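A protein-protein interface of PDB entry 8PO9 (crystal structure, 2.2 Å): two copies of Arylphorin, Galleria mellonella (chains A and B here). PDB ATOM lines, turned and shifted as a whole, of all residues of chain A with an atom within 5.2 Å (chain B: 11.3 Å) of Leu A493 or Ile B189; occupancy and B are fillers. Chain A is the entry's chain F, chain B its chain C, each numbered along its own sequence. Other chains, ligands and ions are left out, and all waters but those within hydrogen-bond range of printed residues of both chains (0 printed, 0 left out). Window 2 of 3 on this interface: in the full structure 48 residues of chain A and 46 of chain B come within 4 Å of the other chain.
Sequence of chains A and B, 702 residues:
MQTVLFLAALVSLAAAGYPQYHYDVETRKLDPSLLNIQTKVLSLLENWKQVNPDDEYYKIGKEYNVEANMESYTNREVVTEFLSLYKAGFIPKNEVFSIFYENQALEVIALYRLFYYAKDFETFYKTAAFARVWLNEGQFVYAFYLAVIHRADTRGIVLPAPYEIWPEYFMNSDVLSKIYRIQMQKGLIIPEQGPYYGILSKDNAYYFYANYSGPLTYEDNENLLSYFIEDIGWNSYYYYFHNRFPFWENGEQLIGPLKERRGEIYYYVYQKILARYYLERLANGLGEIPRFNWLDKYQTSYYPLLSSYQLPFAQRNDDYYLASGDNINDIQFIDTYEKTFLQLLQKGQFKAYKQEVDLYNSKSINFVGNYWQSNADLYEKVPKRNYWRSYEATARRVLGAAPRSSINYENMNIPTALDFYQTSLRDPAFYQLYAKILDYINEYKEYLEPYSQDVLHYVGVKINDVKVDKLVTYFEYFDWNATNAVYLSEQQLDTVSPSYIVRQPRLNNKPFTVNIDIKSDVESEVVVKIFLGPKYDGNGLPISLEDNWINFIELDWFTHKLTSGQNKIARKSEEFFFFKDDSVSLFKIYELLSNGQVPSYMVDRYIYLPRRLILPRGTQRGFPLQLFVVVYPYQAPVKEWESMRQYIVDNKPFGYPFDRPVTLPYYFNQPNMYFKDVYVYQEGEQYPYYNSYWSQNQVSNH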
ATOM      1  N   ASN A  47      23.380 -11.006   8.408  1.00  0.00           N
ATOM      2  CA  ASN A  47      22.917  -9.897   9.250  1.00  0.00           C
ATOM      3  C   ASN A  47      24.071  -9.157   9.915  1.00  0.00           C
ATOM      4  O   ASN A  47      24.023  -8.805  11.092  1.00  0.00           O
ATOM      5  CB  ASN A  47      21.891 -10.381  10.274  1.00  0.00           C
ATOM      6  CG  ASN A  47      20.688 -11.008   9.609  1.00  0.00           C
ATOM      7  OD1 ASN A  47      20.485 -12.219   9.682  1.00  0.00           O
ATOM      8  ND2 ASN A  47      19.887 -10.174   8.915  1.00  0.00           N
ATOM      9  N   GLN A  50      24.069  -6.384  12.562  1.00  0.00           N
ATOM     10  CA  GLN A  50      23.751  -6.617  13.960  1.00  0.00           C
ATOM     11  C   GLN A  50      24.720  -7.621  14.566  1.00  0.00           C
ATOM     12  O   GLN A  50      25.324  -8.436  13.865  1.00  0.00           O
ATOM     13  CB  GLN A  50      22.324  -7.142  14.133  1.00  0.00           C
ATOM     14  CG  GLN A  50      21.247  -6.266  13.567  1.00  0.00           C
ATOM     15  CD  GLN A  50      19.887  -6.902  13.724  1.00  0.00           C
ATOM     16  OE1 GLN A  50      19.446  -7.676  12.874  1.00  0.00           O
ATOM     17  NE2 GLN A  50      19.214  -6.583  14.813  1.00  0.00           N
ATOM     18  N   VAL A  51      24.822  -7.581  15.894  1.00  0.00           N
ATOM     19  CA  VAL A  51      25.584  -8.562  16.661  1.00  0.00           C
ATOM     20  C   VAL A  51      24.608  -9.287  17.583  1.00  0.00           C
ATOM     21  O   VAL A  51      23.963  -8.653  18.432  1.00  0.00           O
ATOM     22  CB  VAL A  51      26.711  -7.900  17.468  1.00  0.00           C
ATOM     23  CG1 VAL A  51      27.331  -8.888  18.403  1.00  0.00           C
ATOM     24  CG2 VAL A  51      27.772  -7.294  16.534  1.00  0.00           C
ATOM     25  N   ASN A  52      24.511 -10.622  17.430  1.00  0.00           N
ATOM     26  CA  ASN A  52      23.648 -11.445  18.279  1.00  0.00           C
ATOM     27  C   ASN A  52      24.484 -12.140  19.340  1.00  0.00           C
ATOM     28  O   ASN A  52      25.309 -13.006  19.005  1.00  0.00           O
ATOM     29  CB  ASN A  52      22.881 -12.476  17.459  1.00  0.00           C
ATOM     30  CG  ASN A  52      22.016 -13.407  18.330  1.00  0.00           C
ATOM     31  OD1 ASN A  52      21.839 -13.191  19.532  1.00  0.00           O
ATOM     32  ND2 ASN A  52      21.479 -14.445  17.712  1.00  0.00           N
ATOM     33  N   PRO A  53      24.278 -11.821  20.617  1.00  0.00           N
ATOM     34  CA  PRO A  53      25.103 -12.421  21.673  1.00  0.00           C
ATOM     35  C   PRO A  53      25.002 -13.930  21.753  1.00  0.00           C
ATOM     36  O   PRO A  53      25.900 -14.554  22.323  1.00  0.00           O
ATOM     37  CB  PRO A  53      24.577 -11.754  22.950  1.00  0.00           C
ATOM     38  CG  PRO A  53      23.946 -10.489  22.478  1.00  0.00           C
ATOM     39  CD  PRO A  53      23.359 -10.802  21.143  1.00  0.00           C
ATOM     40  N   LEU A 488      16.607  -7.209  12.646  1.00  0.00           N
ATOM     41  CA  LEU A 488      15.777  -8.313  13.098  1.00  0.00           C
ATOM     42  C   LEU A 488      15.679  -8.311  14.616  1.00  0.00           C
ATOM     43  O   LEU A 488      16.577  -7.822  15.311  1.00  0.00           O
ATOM     44  CB  LEU A 488      16.364  -9.636  12.610  1.00  0.00           C
ATOM     45  CG  LEU A 488      16.435  -9.798  11.089  1.00  0.00           C
ATOM     46  CD1 LEU A 488      17.156 -11.078  10.734  1.00  0.00           C
ATOM     47  CD2 LEU A 488      15.030  -9.819  10.505  1.00  0.00           C
ATOM     48  N   SER A 489      14.573  -8.863  15.127  1.00  0.00           N
ATOM     49  CA  SER A 489      14.395  -8.995  16.563  1.00  0.00           C
ATOM     50  C   SER A 489      15.275 -10.119  17.117  1.00  0.00           C
ATOM     51  O   SER A 489      15.831 -10.936  16.378  1.00  0.00           O
ATOM     52  CB  SER A 489      12.926  -9.251  16.909  1.00  0.00           C
ATOM     53  OG  SER A 489      12.505 -10.538  16.486  1.00  0.00           O
ATOM     54  N   GLU A 490      15.412 -10.137  18.449  1.00  0.00           N
ATOM     55  CA  GLU A 490      16.128 -11.228  19.096  1.00  0.00           C
ATOM     56  C   GLU A 490      15.430 -12.556  18.837  1.00  0.00           C
ATOM     57  O   GLU A 490      16.083 -13.563  18.544  1.00  0.00           O
ATOM     58  CB  GLU A 490      16.255 -10.961  20.601  1.00  0.00           C
ATOM     59  CG  GLU A 490      16.930 -12.080  21.394  1.00  0.00           C
ATOM     60  CD  GLU A 490      18.422 -12.236  21.084  1.00  0.00           C
ATOM     61  OE1 GLU A 490      19.004 -11.352  20.417  1.00  0.00           O
ATOM     62  OE2 GLU A 490      19.019 -13.253  21.503  1.00  0.00           O
ATOM     63  N   GLN A 491      14.099 -12.556  18.877  1.00  0.00           N
ATOM     64  CA  GLN A 491      13.334 -13.753  18.536  1.00  0.00           C
ATOM     65  C   GLN A 491      13.668 -14.254  17.128  1.00  0.00           C
ATOM     66  O   GLN A 491      13.862 -15.458  16.925  1.00  0.00           O
ATOM     67  CB  GLN A 491      11.849 -13.423  18.666  1.00  0.00           C
ATOM     68  CG  GLN A 491      10.858 -14.455  18.184  1.00  0.00           C
ATOM     69  CD  GLN A 491       9.431 -14.011  18.477  1.00  0.00           C
ATOM     70  OE1 GLN A 491       9.196 -12.853  18.839  1.00  0.00           O
ATOM     71  NE2 GLN A 491       8.470 -14.904  18.258  1.00  0.00           N
ATOM     72  N   GLN A 492      13.752 -13.343  16.144  1.00  0.00           N
ATOM     73  CA  GLN A 492      14.058 -13.746  14.768  1.00  0.00           C
ATOM     74  C   GLN A 492      15.519 -14.148  14.586  1.00  0.00           C
ATOM     75  O   GLN A 492      15.819 -15.080  13.831  1.00  0.00           O
ATOM     76  CB  GLN A 492      13.721 -12.617  13.801  1.00  0.00           C
ATOM     77  CG  GLN A 492      12.250 -12.332  13.657  1.00  0.00           C
ATOM     78  CD  GLN A 492      12.013 -10.955  13.086  1.00  0.00           C
ATOM     79  OE1 GLN A 492      12.879 -10.088  13.175  1.00  0.00           O
ATOM     80  NE2 GLN A 492      10.833 -10.737  12.519  1.00  0.00           N
ATOM     81  N   LEU A 493      16.445 -13.446  15.245  1.00  0.00           N
ATOM     82  CA  LEU A 493      17.863 -13.765  15.087  1.00  0.00           C
ATOM     83  C   LEU A 493      18.189 -15.158  15.617  1.00  0.00           C
ATOM     84  O   LEU A 493      19.044 -15.858  15.062  1.00  0.00           O
ATOM     85  CB  LEU A 493      18.724 -12.714  15.789  1.00  0.00           C
ATOM     86  CG  LEU A 493      18.788 -11.312  15.173  1.00  0.00           C
ATOM     87  CD1 LEU A 493      19.363 -10.320  16.186  1.00  0.00           C
ATOM     88  CD2 LEU A 493      19.576 -11.290  13.867  1.00  0.00           C
ATOM     89  N   ASP A 494      17.523 -15.579  16.690  1.00  0.00           N
ATOM     90  CA  ASP A 494      17.806 -16.886  17.273  1.00  0.00           C
ATOM     91  C   ASP A 494      17.135 -18.011  16.494  1.00  0.00           C
ATOM     92  O   ASP A 494      17.680 -19.117  16.412  1.00  0.00           O
ATOM     93  CB  ASP A 494      17.373 -16.902  18.740  1.00  0.00           C
ATOM     94  CG  ASP A 494      18.310 -16.100  19.633  1.00  0.00           C
ATOM     95  OD1 ASP A 494      19.464 -15.865  19.218  1.00  0.00           O
ATOM     96  OD2 ASP A 494      17.899 -15.707  20.748  1.00  0.00           O
ATOM     97  N   THR A 495      15.954 -17.757  15.950  1.00  0.00           N
ATOM     98  CA  THR A 495      15.250 -18.635  15.035  1.00  0.00           C
ATOM     99  C   THR A 495      15.575 -18.165  13.617  1.00  0.00           C
ATOM    100  O   THR A 495      16.594 -17.507  13.394  1.00  0.00           O
ATOM    101  CB  THR A 495      13.753 -18.629  15.348  1.00  0.00           C
ATOM    102  OG1 THR A 495      13.181 -17.386  14.940  1.00  0.00           O
ATOM    103  CG2 THR A 495      13.539 -18.796  16.849  1.00  0.00           C
ATOM    104  N   LYS B 178      17.135   5.639  14.600  1.00  0.00           N
ATOM    105  CA  LYS B 178      17.264   4.855  15.828  1.00  0.00           C
ATOM    106  C   LYS B 178      15.900   4.376  16.310  1.00  0.00           C
ATOM    107  O   LYS B 178      15.747   3.222  16.713  1.00  0.00           O
ATOM    108  CB  LYS B 178      17.950   5.669  16.927  1.00  0.00           C
ATOM    109  CG  LYS B 178      19.430   5.931  16.764  1.00  0.00           C
ATOM    110  CD  LYS B 178      19.845   6.931  17.817  1.00  0.00           C
ATOM    111  CE  LYS B 178      21.328   7.185  17.819  1.00  0.00           C
ATOM    112  NZ  LYS B 178      21.650   8.270  18.781  1.00  0.00           N
ATOM    113  N   TYR B 180      13.094   3.903  14.494  1.00  0.00           N
ATOM    114  CA  TYR B 180      12.623   2.843  13.599  1.00  0.00           C
ATOM    115  C   TYR B 180      13.352   1.530  13.851  1.00  0.00           C
ATOM    116  O   TYR B 180      12.754   0.448  13.773  1.00  0.00           O
ATOM    117  CB  TYR B 180      12.821   3.230  12.131  1.00  0.00           C
ATOM    118  CG  TYR B 180      12.024   4.413  11.643  1.00  0.00           C
ATOM    119  CD1 TYR B 180      10.781   4.721  12.182  1.00  0.00           C
ATOM    120  CD2 TYR B 180      12.515   5.216  10.617  1.00  0.00           C
ATOM    121  CE1 TYR B 180      10.057   5.809  11.719  1.00  0.00           C
ATOM    122  CE2 TYR B 180      11.800   6.301  10.149  1.00  0.00           C
ATOM    123  CZ  TYR B 180      10.575   6.593  10.701  1.00  0.00           C
ATOM    124  OH  TYR B 180       9.871   7.675  10.220  1.00  0.00           O
ATOM    125  N   ARG B 181      14.657   1.599  14.107  1.00  0.00           N
ATOM    126  CA  ARG B 181      15.407   0.369  14.334  1.00  0.00           C
ATOM    127  C   ARG B 181      14.914  -0.356  15.582  1.00  0.00           C
ATOM    128  O   ARG B 181      14.771  -1.586  15.577  1.00  0.00           O
ATOM    129  CB  ARG B 181      16.899   0.669  14.441  1.00  0.00           C
ATOM    130  CG  ARG B 181      17.704  -0.540  14.745  1.00  0.00           C
ATOM    131  CD  ARG B 181      19.152  -0.262  14.597  1.00  0.00           C
ATOM    132  NE  ARG B 181      19.923  -1.408  15.055  1.00  0.00           N
ATOM    133  CZ  ARG B 181      21.236  -1.512  14.929  1.00  0.00           C
ATOM    134  NH1 ARG B 181      21.955  -0.537  14.381  1.00  0.00           N
ATOM    135  NH2 ARG B 181      21.841  -2.622  15.345  1.00  0.00           N
ATOM    136  N   ILE B 182      14.645   0.388  16.659  1.00  0.00           N
ATOM    137  CA  ILE B 182      14.108  -0.242  17.864  1.00  0.00           C
ATOM    138  C   ILE B 182      12.755  -0.887  17.574  1.00  0.00           C
ATOM    139  O   ILE B 182      12.474  -2.009  18.023  1.00  0.00           O
ATOM    140  CB  ILE B 182      14.019   0.767  19.020  1.00  0.00           C
ATOM    141  CG1 ILE B 182      15.393   1.372  19.324  1.00  0.00           C
ATOM    142  CG2 ILE B 182      13.485   0.083  20.248  1.00  0.00           C
ATOM    143  CD1 ILE B 182      16.492   0.350  19.593  1.00  0.00           C
ATOM    144  N   GLN B 183      11.890  -0.198  16.824  1.00  0.00           N
ATOM    145  CA  GLN B 183      10.614  -0.816  16.475  1.00  0.00           C
ATOM    146  C   GLN B 183      10.823  -2.070  15.635  1.00  0.00           C
ATOM    147  O   GLN B 183      10.166  -3.091  15.861  1.00  0.00           O
ATOM    148  CB  GLN B 183       9.711   0.170  15.743  1.00  0.00           C
ATOM    149  CG  GLN B 183       8.420  -0.474  15.231  1.00  0.00           C
ATOM    150  CD  GLN B 183       7.502  -0.955  16.350  1.00  0.00           C
ATOM    151  OE1 GLN B 183       7.634  -0.538  17.503  1.00  0.00           O
ATOM    152  NE2 GLN B 183       6.576  -1.847  16.014  1.00  0.00           N
ATOM    153  N   MET B 184      11.744  -2.016  14.668  1.00  0.00           N
ATOM    154  CA  MET B 184      12.061  -3.206  13.881  1.00  0.00           C
ATOM    155  C   MET B 184      12.576  -4.336  14.767  1.00  0.00           C
ATOM    156  O   MET B 184      12.212  -5.508  14.578  1.00  0.00           O
ATOM    157  CB  MET B 184      13.088  -2.864  12.798  1.00  0.00           C
ATOM    158  CG  MET B 184      12.506  -2.261  11.535  1.00  0.00           C
ATOM    159  SD  MET B 184      13.719  -2.175  10.195  1.00  0.00           S
ATOM    160  CE  MET B 184      14.370  -0.525  10.400  1.00  0.00           C
ATOM    161  N   GLN B 185      13.441  -4.012  15.725  1.00  0.00           N
ATOM    162  CA  GLN B 185      14.009  -5.061  16.553  1.00  0.00           C
ATOM    163  C   GLN B 185      13.101  -5.483  17.699  1.00  0.00           C
ATOM    164  O   GLN B 185      13.410  -6.481  18.362  1.00  0.00           O
ATOM    165  CB  GLN B 185      15.359  -4.633  17.118  1.00  0.00           C
ATOM    166  CG  GLN B 185      16.430  -4.416  16.086  1.00  0.00           C
ATOM    167  CD  GLN B 185      17.706  -3.861  16.679  1.00  0.00           C
ATOM    168  OE1 GLN B 185      18.743  -3.836  16.016  1.00  0.00           O
ATOM    169  NE2 GLN B 185      17.647  -3.427  17.939  1.00  0.00           N
ATOM    170  N   LYS B 186      12.008  -4.756  17.954  1.00  0.00           N
ATOM    171  CA  LYS B 186      11.175  -4.987  19.139  1.00  0.00           C
ATOM    172  C   LYS B 186      12.002  -4.931  20.431  1.00  0.00           C
ATOM    173  O   LYS B 186      11.880  -5.773  21.321  1.00  0.00           O
ATOM    174  CB  LYS B 186      10.412  -6.304  19.012  1.00  0.00           C
ATOM    175  CG  LYS B 186       9.370  -6.331  17.864  1.00  0.00           C
ATOM    176  CD  LYS B 186       8.435  -5.086  17.895  1.00  0.00           C
ATOM    177  CE  LYS B 186       7.336  -5.114  16.803  1.00  0.00           C
ATOM    178  NZ  LYS B 186       7.855  -4.924  15.421  1.00  0.00           N
ATOM    179  N   GLY B 187      12.871  -3.922  20.528  1.00  0.00           N
ATOM    180  CA  GLY B 187      13.712  -3.651  21.675  1.00  0.00           C
ATOM    181  C   GLY B 187      15.168  -3.539  21.269  1.00  0.00           C
ATOM    182  O   GLY B 187      15.508  -3.440  20.085  1.00  0.00           O
ATOM    183  N   LEU B 188      16.039  -3.538  22.268  1.00  0.00           N
ATOM    184  CA  LEU B 188      17.482  -3.521  22.080  1.00  0.00           C
ATOM    185  C   LEU B 188      17.979  -4.954  22.147  1.00  0.00           C
ATOM    186  O   LEU B 188      17.625  -5.683  23.073  1.00  0.00           O
ATOM    187  CB  LEU B 188      18.164  -2.671  23.157  1.00  0.00           C
ATOM    188  CG  LEU B 188      17.882  -1.162  23.130  1.00  0.00           C
ATOM    189  CD1 LEU B 188      17.834  -0.556  24.528  1.00  0.00           C
ATOM    190  CD2 LEU B 188      18.948  -0.483  22.310  1.00  0.00           C
ATOM    191  N   ILE B 189      18.801  -5.357  21.175  1.00  0.00           N
ATOM    192  CA  ILE B 189      19.355  -6.710  21.214  1.00  0.00           C
ATOM    193  C   ILE B 189      20.257  -6.870  22.432  1.00  0.00           C
ATOM    194  O   ILE B 189      20.251  -7.914  23.097  1.00  0.00           O
ATOM    195  CB  ILE B 189      20.096  -7.040  19.907  1.00  0.00           C
ATOM    196  CG1 ILE B 189      19.185  -6.808  18.693  1.00  0.00           C
ATOM    197  CG2 ILE B 189      20.566  -8.473  19.938  1.00  0.00           C
ATOM    198  CD1 ILE B 189      17.926  -7.662  18.699  1.00  0.00           C
ATOM    199  N   ILE B 190      21.043  -5.840  22.738  1.00  0.00           N
ATOM    200  CA  ILE B 190      21.889  -5.790  23.928  1.00  0.00           C
ATOM    201  C   ILE B 190      21.475  -4.563  24.737  1.00  0.00           C
ATOM    202  O   ILE B 190      21.999  -3.460  24.503  1.00  0.00           O
ATOM    203  CB  ILE B 190      23.380  -5.741  23.563  1.00  0.00           C
ATOM    204  CG1 ILE B 190      23.735  -6.889  22.623  1.00  0.00           C
ATOM    205  CG2 ILE B 190      24.246  -5.768  24.822  1.00  0.00           C
ATOM    206  CD1 ILE B 190      25.181  -6.863  22.157  1.00  0.00           C
ATOM    207  N   PRO B 191      20.527  -4.698  25.674  1.00  0.00           N
ATOM    208  CA  PRO B 191      19.944  -3.498  26.308  1.00  0.00           C
ATOM    209  C   PRO B 191      20.955  -2.593  26.983  1.00  0.00           C
ATOM    210  O   PRO B 191      20.814  -1.367  26.923  1.00  0.00           O
ATOM    211  CB  PRO B 191      18.963  -4.091  27.329  1.00  0.00           C
ATOM    212  CG  PRO B 191      18.563  -5.401  26.721  1.00  0.00           C
ATOM    213  CD  PRO B 191      19.820  -5.930  26.063  1.00  0.00           C
ATOM    214  N   GLU B 192      21.994  -3.155  27.594  1.00  0.00           N
ATOM    215  CA  GLU B 192      22.949  -2.305  28.284  1.00  0.00           C
ATOM    216  C   GLU B 192      23.748  -1.427  27.330  1.00  0.00           C
ATOM    217  O   GLU B 192      24.261  -0.393  27.757  1.00  0.00           O
ATOM    218  CB  GLU B 192      23.900  -3.153  29.118  1.00  0.00           C
ATOM    219  CG  GLU B 192      24.873  -3.952  28.301  1.00  0.00           C
ATOM    220  CD  GLU B 192      25.735  -4.831  29.170  1.00  0.00           C
ATOM    221  OE1 GLU B 192      25.365  -4.976  30.348  1.00  0.00           O
ATOM    222  OE2 GLU B 192      26.777  -5.335  28.693  1.00  0.00           O
ATOM    223  N   GLN B 193      23.832  -1.782  26.049  1.00  0.00           N
ATOM    224  CA  GLN B 193      24.571  -0.960  25.101  1.00  0.00           C
ATOM    225  C   GLN B 193      23.804   0.282  24.680  1.00  0.00           C
ATOM    226  O   GLN B 193      24.400   1.190  24.092  1.00  0.00           O
ATOM    227  CB  GLN B 193      24.938  -1.786  23.877  1.00  0.00           C
ATOM    228  CG  GLN B 193      26.091  -2.735  24.134  1.00  0.00           C
ATOM    229  CD  GLN B 193      26.725  -3.243  22.863  1.00  0.00           C
ATOM    230  OE1 GLN B 193      26.072  -3.328  21.818  1.00  0.00           O
ATOM    231  NE2 GLN B 193      27.987  -3.657  22.957  1.00  0.00           N
ATOM    232  N   GLY B 194      22.504   0.337  24.955  1.00  0.00           N
ATOM    233  CA  GLY B 194      21.676   1.446  24.550  1.00  0.00           C
ATOM    234  C   GLY B 194      22.227   2.814  24.923  1.00  0.00           C
ATOM    235  O   GLY B 194      22.341   3.705  24.072  1.00  0.00           O
ATOM    236  N   PRO B 195      22.576   3.015  26.200  1.00  0.00           N
ATOM    237  CA  PRO B 195      23.069   4.339  26.619  1.00  0.00           C
ATOM    238  C   PRO B 195      24.294   4.837  25.861  1.00  0.00           C
ATOM    239  O   PRO B 195      24.436   6.052  25.689  1.00  0.00           O
ATOM    240  CB  PRO B 195      23.376   4.130  28.109  1.00  0.00           C
ATOM    241  CG  PRO B 195      22.432   3.060  28.530  1.00  0.00           C
ATOM    242  CD  PRO B 195      22.350   2.130  27.361  1.00  0.00           C
ATOM    243  N   TYR B 197      24.762   4.743  22.837  1.00  0.00           N
ATOM    244  CA  TYR B 197      24.211   5.272  21.606  1.00  0.00           C
ATOM    245  C   TYR B 197      23.040   6.194  21.885  1.00  0.00           C
ATOM    246  O   TYR B 197      22.186   6.394  21.015  1.00  0.00           O
ATOM    247  CB  TYR B 197      23.821   4.104  20.701  1.00  0.00           C
ATOM    248  CG  TYR B 197      25.030   3.273  20.369  1.00  0.00           C
ATOM    249  CD1 TYR B 197      25.868   3.635  19.321  1.00  0.00           C
ATOM    250  CD2 TYR B 197      25.389   2.181  21.153  1.00  0.00           C
ATOM    251  CE1 TYR B 197      26.998   2.907  19.024  1.00  0.00           C
ATOM    252  CE2 TYR B 197      26.528   1.454  20.878  1.00  0.00           C
ATOM    253  CZ  TYR B 197      27.329   1.824  19.803  1.00  0.00           C
ATOM    254  OH  TYR B 197      28.463   1.111  19.503  1.00  0.00           O
ATOM    255  N   ILE B 199      20.414   5.854  24.037  1.00  0.00           N
ATOM    256  CA  ILE B 199      19.107   5.206  24.161  1.00  0.00           C
ATOM    257  C   ILE B 199      18.928   4.661  25.578  1.00  0.00           C
ATOM    258  O   ILE B 199      19.715   3.827  26.038  1.00  0.00           O
ATOM    259  CB  ILE B 199      18.926   4.085  23.122  1.00  0.00           C
ATOM    260  CG1 ILE B 199      19.049   4.639  21.695  1.00  0.00           C
ATOM    261  CG2 ILE B 199      17.583   3.387  23.323  1.00  0.00           C
ATOM    262  CD1 ILE B 199      18.949   3.580  20.602  1.00  0.00           C
ATOM    263  N   SER B 201      16.009   2.856  28.318  1.00  0.00           N
ATOM    264  CA  SER B 201      14.839   1.989  28.340  1.00  0.00           C
ATOM    265  C   SER B 201      14.278   1.925  29.753  1.00  0.00           C
ATOM    266  O   SER B 201      15.024   1.667  30.700  1.00  0.00           O
ATOM    267  CB  SER B 201      15.196   0.581  27.847  1.00  0.00           C
ATOM    268  OG  SER B 201      14.045  -0.236  27.764  1.00  0.00           O
ATOM    269  N   TYR B 206      11.069   3.852  25.458  1.00  0.00           N
ATOM    270  CA  TYR B 206      12.433   4.065  24.999  1.00  0.00           C
ATOM    271  C   TYR B 206      12.703   5.555  24.860  1.00  0.00           C
ATOM    272  O   TYR B 206      11.865   6.296  24.341  1.00  0.00           O
ATOM    273  CB  TYR B 206      12.687   3.341  23.681  1.00  0.00           C
ATOM    274  CG  TYR B 206      12.569   1.847  23.812  1.00  0.00           C
ATOM    275  CD1 TYR B 206      13.657   1.087  24.197  1.00  0.00           C
ATOM    276  CD2 TYR B 206      11.370   1.196  23.545  1.00  0.00           C
ATOM    277  CE1 TYR B 206      13.560  -0.279  24.322  1.00  0.00           C
ATOM    278  CE2 TYR B 206      11.261  -0.165  23.650  1.00  0.00           C
ATOM    279  CZ  TYR B 206      12.357  -0.905  24.047  1.00  0.00           C
ATOM    280  OH  TYR B 206      12.251  -2.278  24.166  1.00  0.00           O
ATOM    281  N   PHE B 208      15.269   8.553  23.502  1.00  0.00           N
ATOM    282  CA  PHE B 208      16.257   8.848  22.471  1.00  0.00           C
ATOM    283  C   PHE B 208      16.784  10.265  22.671  1.00  0.00           C
ATOM    284  O   PHE B 208      16.071  11.246  22.412  1.00  0.00           O
ATOM    285  CB  PHE B 208      15.644   8.683  21.079  1.00  0.00           C
ATOM    286  CG  PHE B 208      15.067   7.309  20.834  1.00  0.00           C
ATOM    287  CD1 PHE B 208      13.805   6.973  21.316  1.00  0.00           C
ATOM    288  CD2 PHE B 208      15.797   6.345  20.145  1.00  0.00           C
ATOM    289  CE1 PHE B 208      13.271   5.714  21.108  1.00  0.00           C
ATOM    290  CE2 PHE B 208      15.273   5.076  19.929  1.00  0.00           C
ATOM    291  CZ  PHE B 208      14.001   4.764  20.411  1.00  0.00           C
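Of the 13 printed residues of chain A, 7 touch a printed residue of chain B. Among the printed residues, 11 pairs touch across the chains.
Of the printed residues of chain B, Val A51 touches Ile B189 (3.7 Å). No residue of chain B comes within 4 Å of Asn A52. Of the printed residues of chain B, Pro A53 touches Ile B189 and Ile B190. Leu A488 touches just these residues of chain B: Gln B185 (3.5 Å) and Ile B189 (3.7 Å). Of chain B, only Gln B185 and Ile B189 come within 4 Å of Ser A489. Glu A490 touches just one residue of chain B: Ile B189. Leu A493 touches just one residue of chain B: Ile B189. No residue of chain B comes within 4 Å of Thr A495. Of the printed residues of chain A, Gln B185 touches Gln A50 (3.0 Å), Leu A488 (3.5 Å) and Ser A489 (3.2 Å). Lys B186 touches none of the printed residues of chain A. Printed residues of chain A within 4 Å of Ile B189: Gln A50, Val A51, Pro A53, Leu A488, Ser A489, Glu A490 and Leu A493. Of the printed residues of chain A, Ile B190 touches Pro A53. Pro B191 touches none of the printed residues of chain A. The nearest residue of chain A that does not touch Ile B189 is Asn A52 (4.6 Å). The nearest printed residue of chain A that does not touch Gln B185 is Glu A490 (4.2 Å).
The side-chain carboxylate (OE2) of Glu A490 sits close to the side-chain amide oxygen (OD1) of Asn A52, at 3.4 Å. The side-chain amide oxygen (OE1) of Gln A50 sits at hydrogen-bond distance from the backbone NH (N) of Leu A488 (2.9 Å). OE1 of Gln A492 lies within hydrogen-bond range of N of Ser A489, 2.9 Å away. O of Gly B187 sits at hydrogen-bond distance from NE2 of Gln B185 (3.0 Å). The guanidinium group of Arg B181 sits at hydrogen-bond distance from the side-chain amide oxygen of Gln B185, at 2.9 Å.
No position is printed for both chains.
OE1 of Gln B185 sits at hydrogen-bond distance from NE2 of Gln A50 (3.0 Å).
NE2 of Gln A50 touches CG1 of Ile B189, at 3.9 Å. CG2 of Ile B189 touches O of Val A51 (3.7 Å). Ile B189 touches Pro A53. CG of Pro A53 touches CG1 of Ile B190, 3.6 Å away. Gln B185 touches Leu A488 (CG to O, 3.5 Å). Ile B189 touches Leu A488 (CD1 to O, 3.7 Å). O of Gln B185 touches CB of Ser A489, at 3.2 Å. Ser A489 touches Ile B189. OE1 of Glu A490 touches CG2 of Ile B189, 3.3 Å away. CD1 of Ile B189 touches CD1 of Leu A493, 3.9 Å away.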
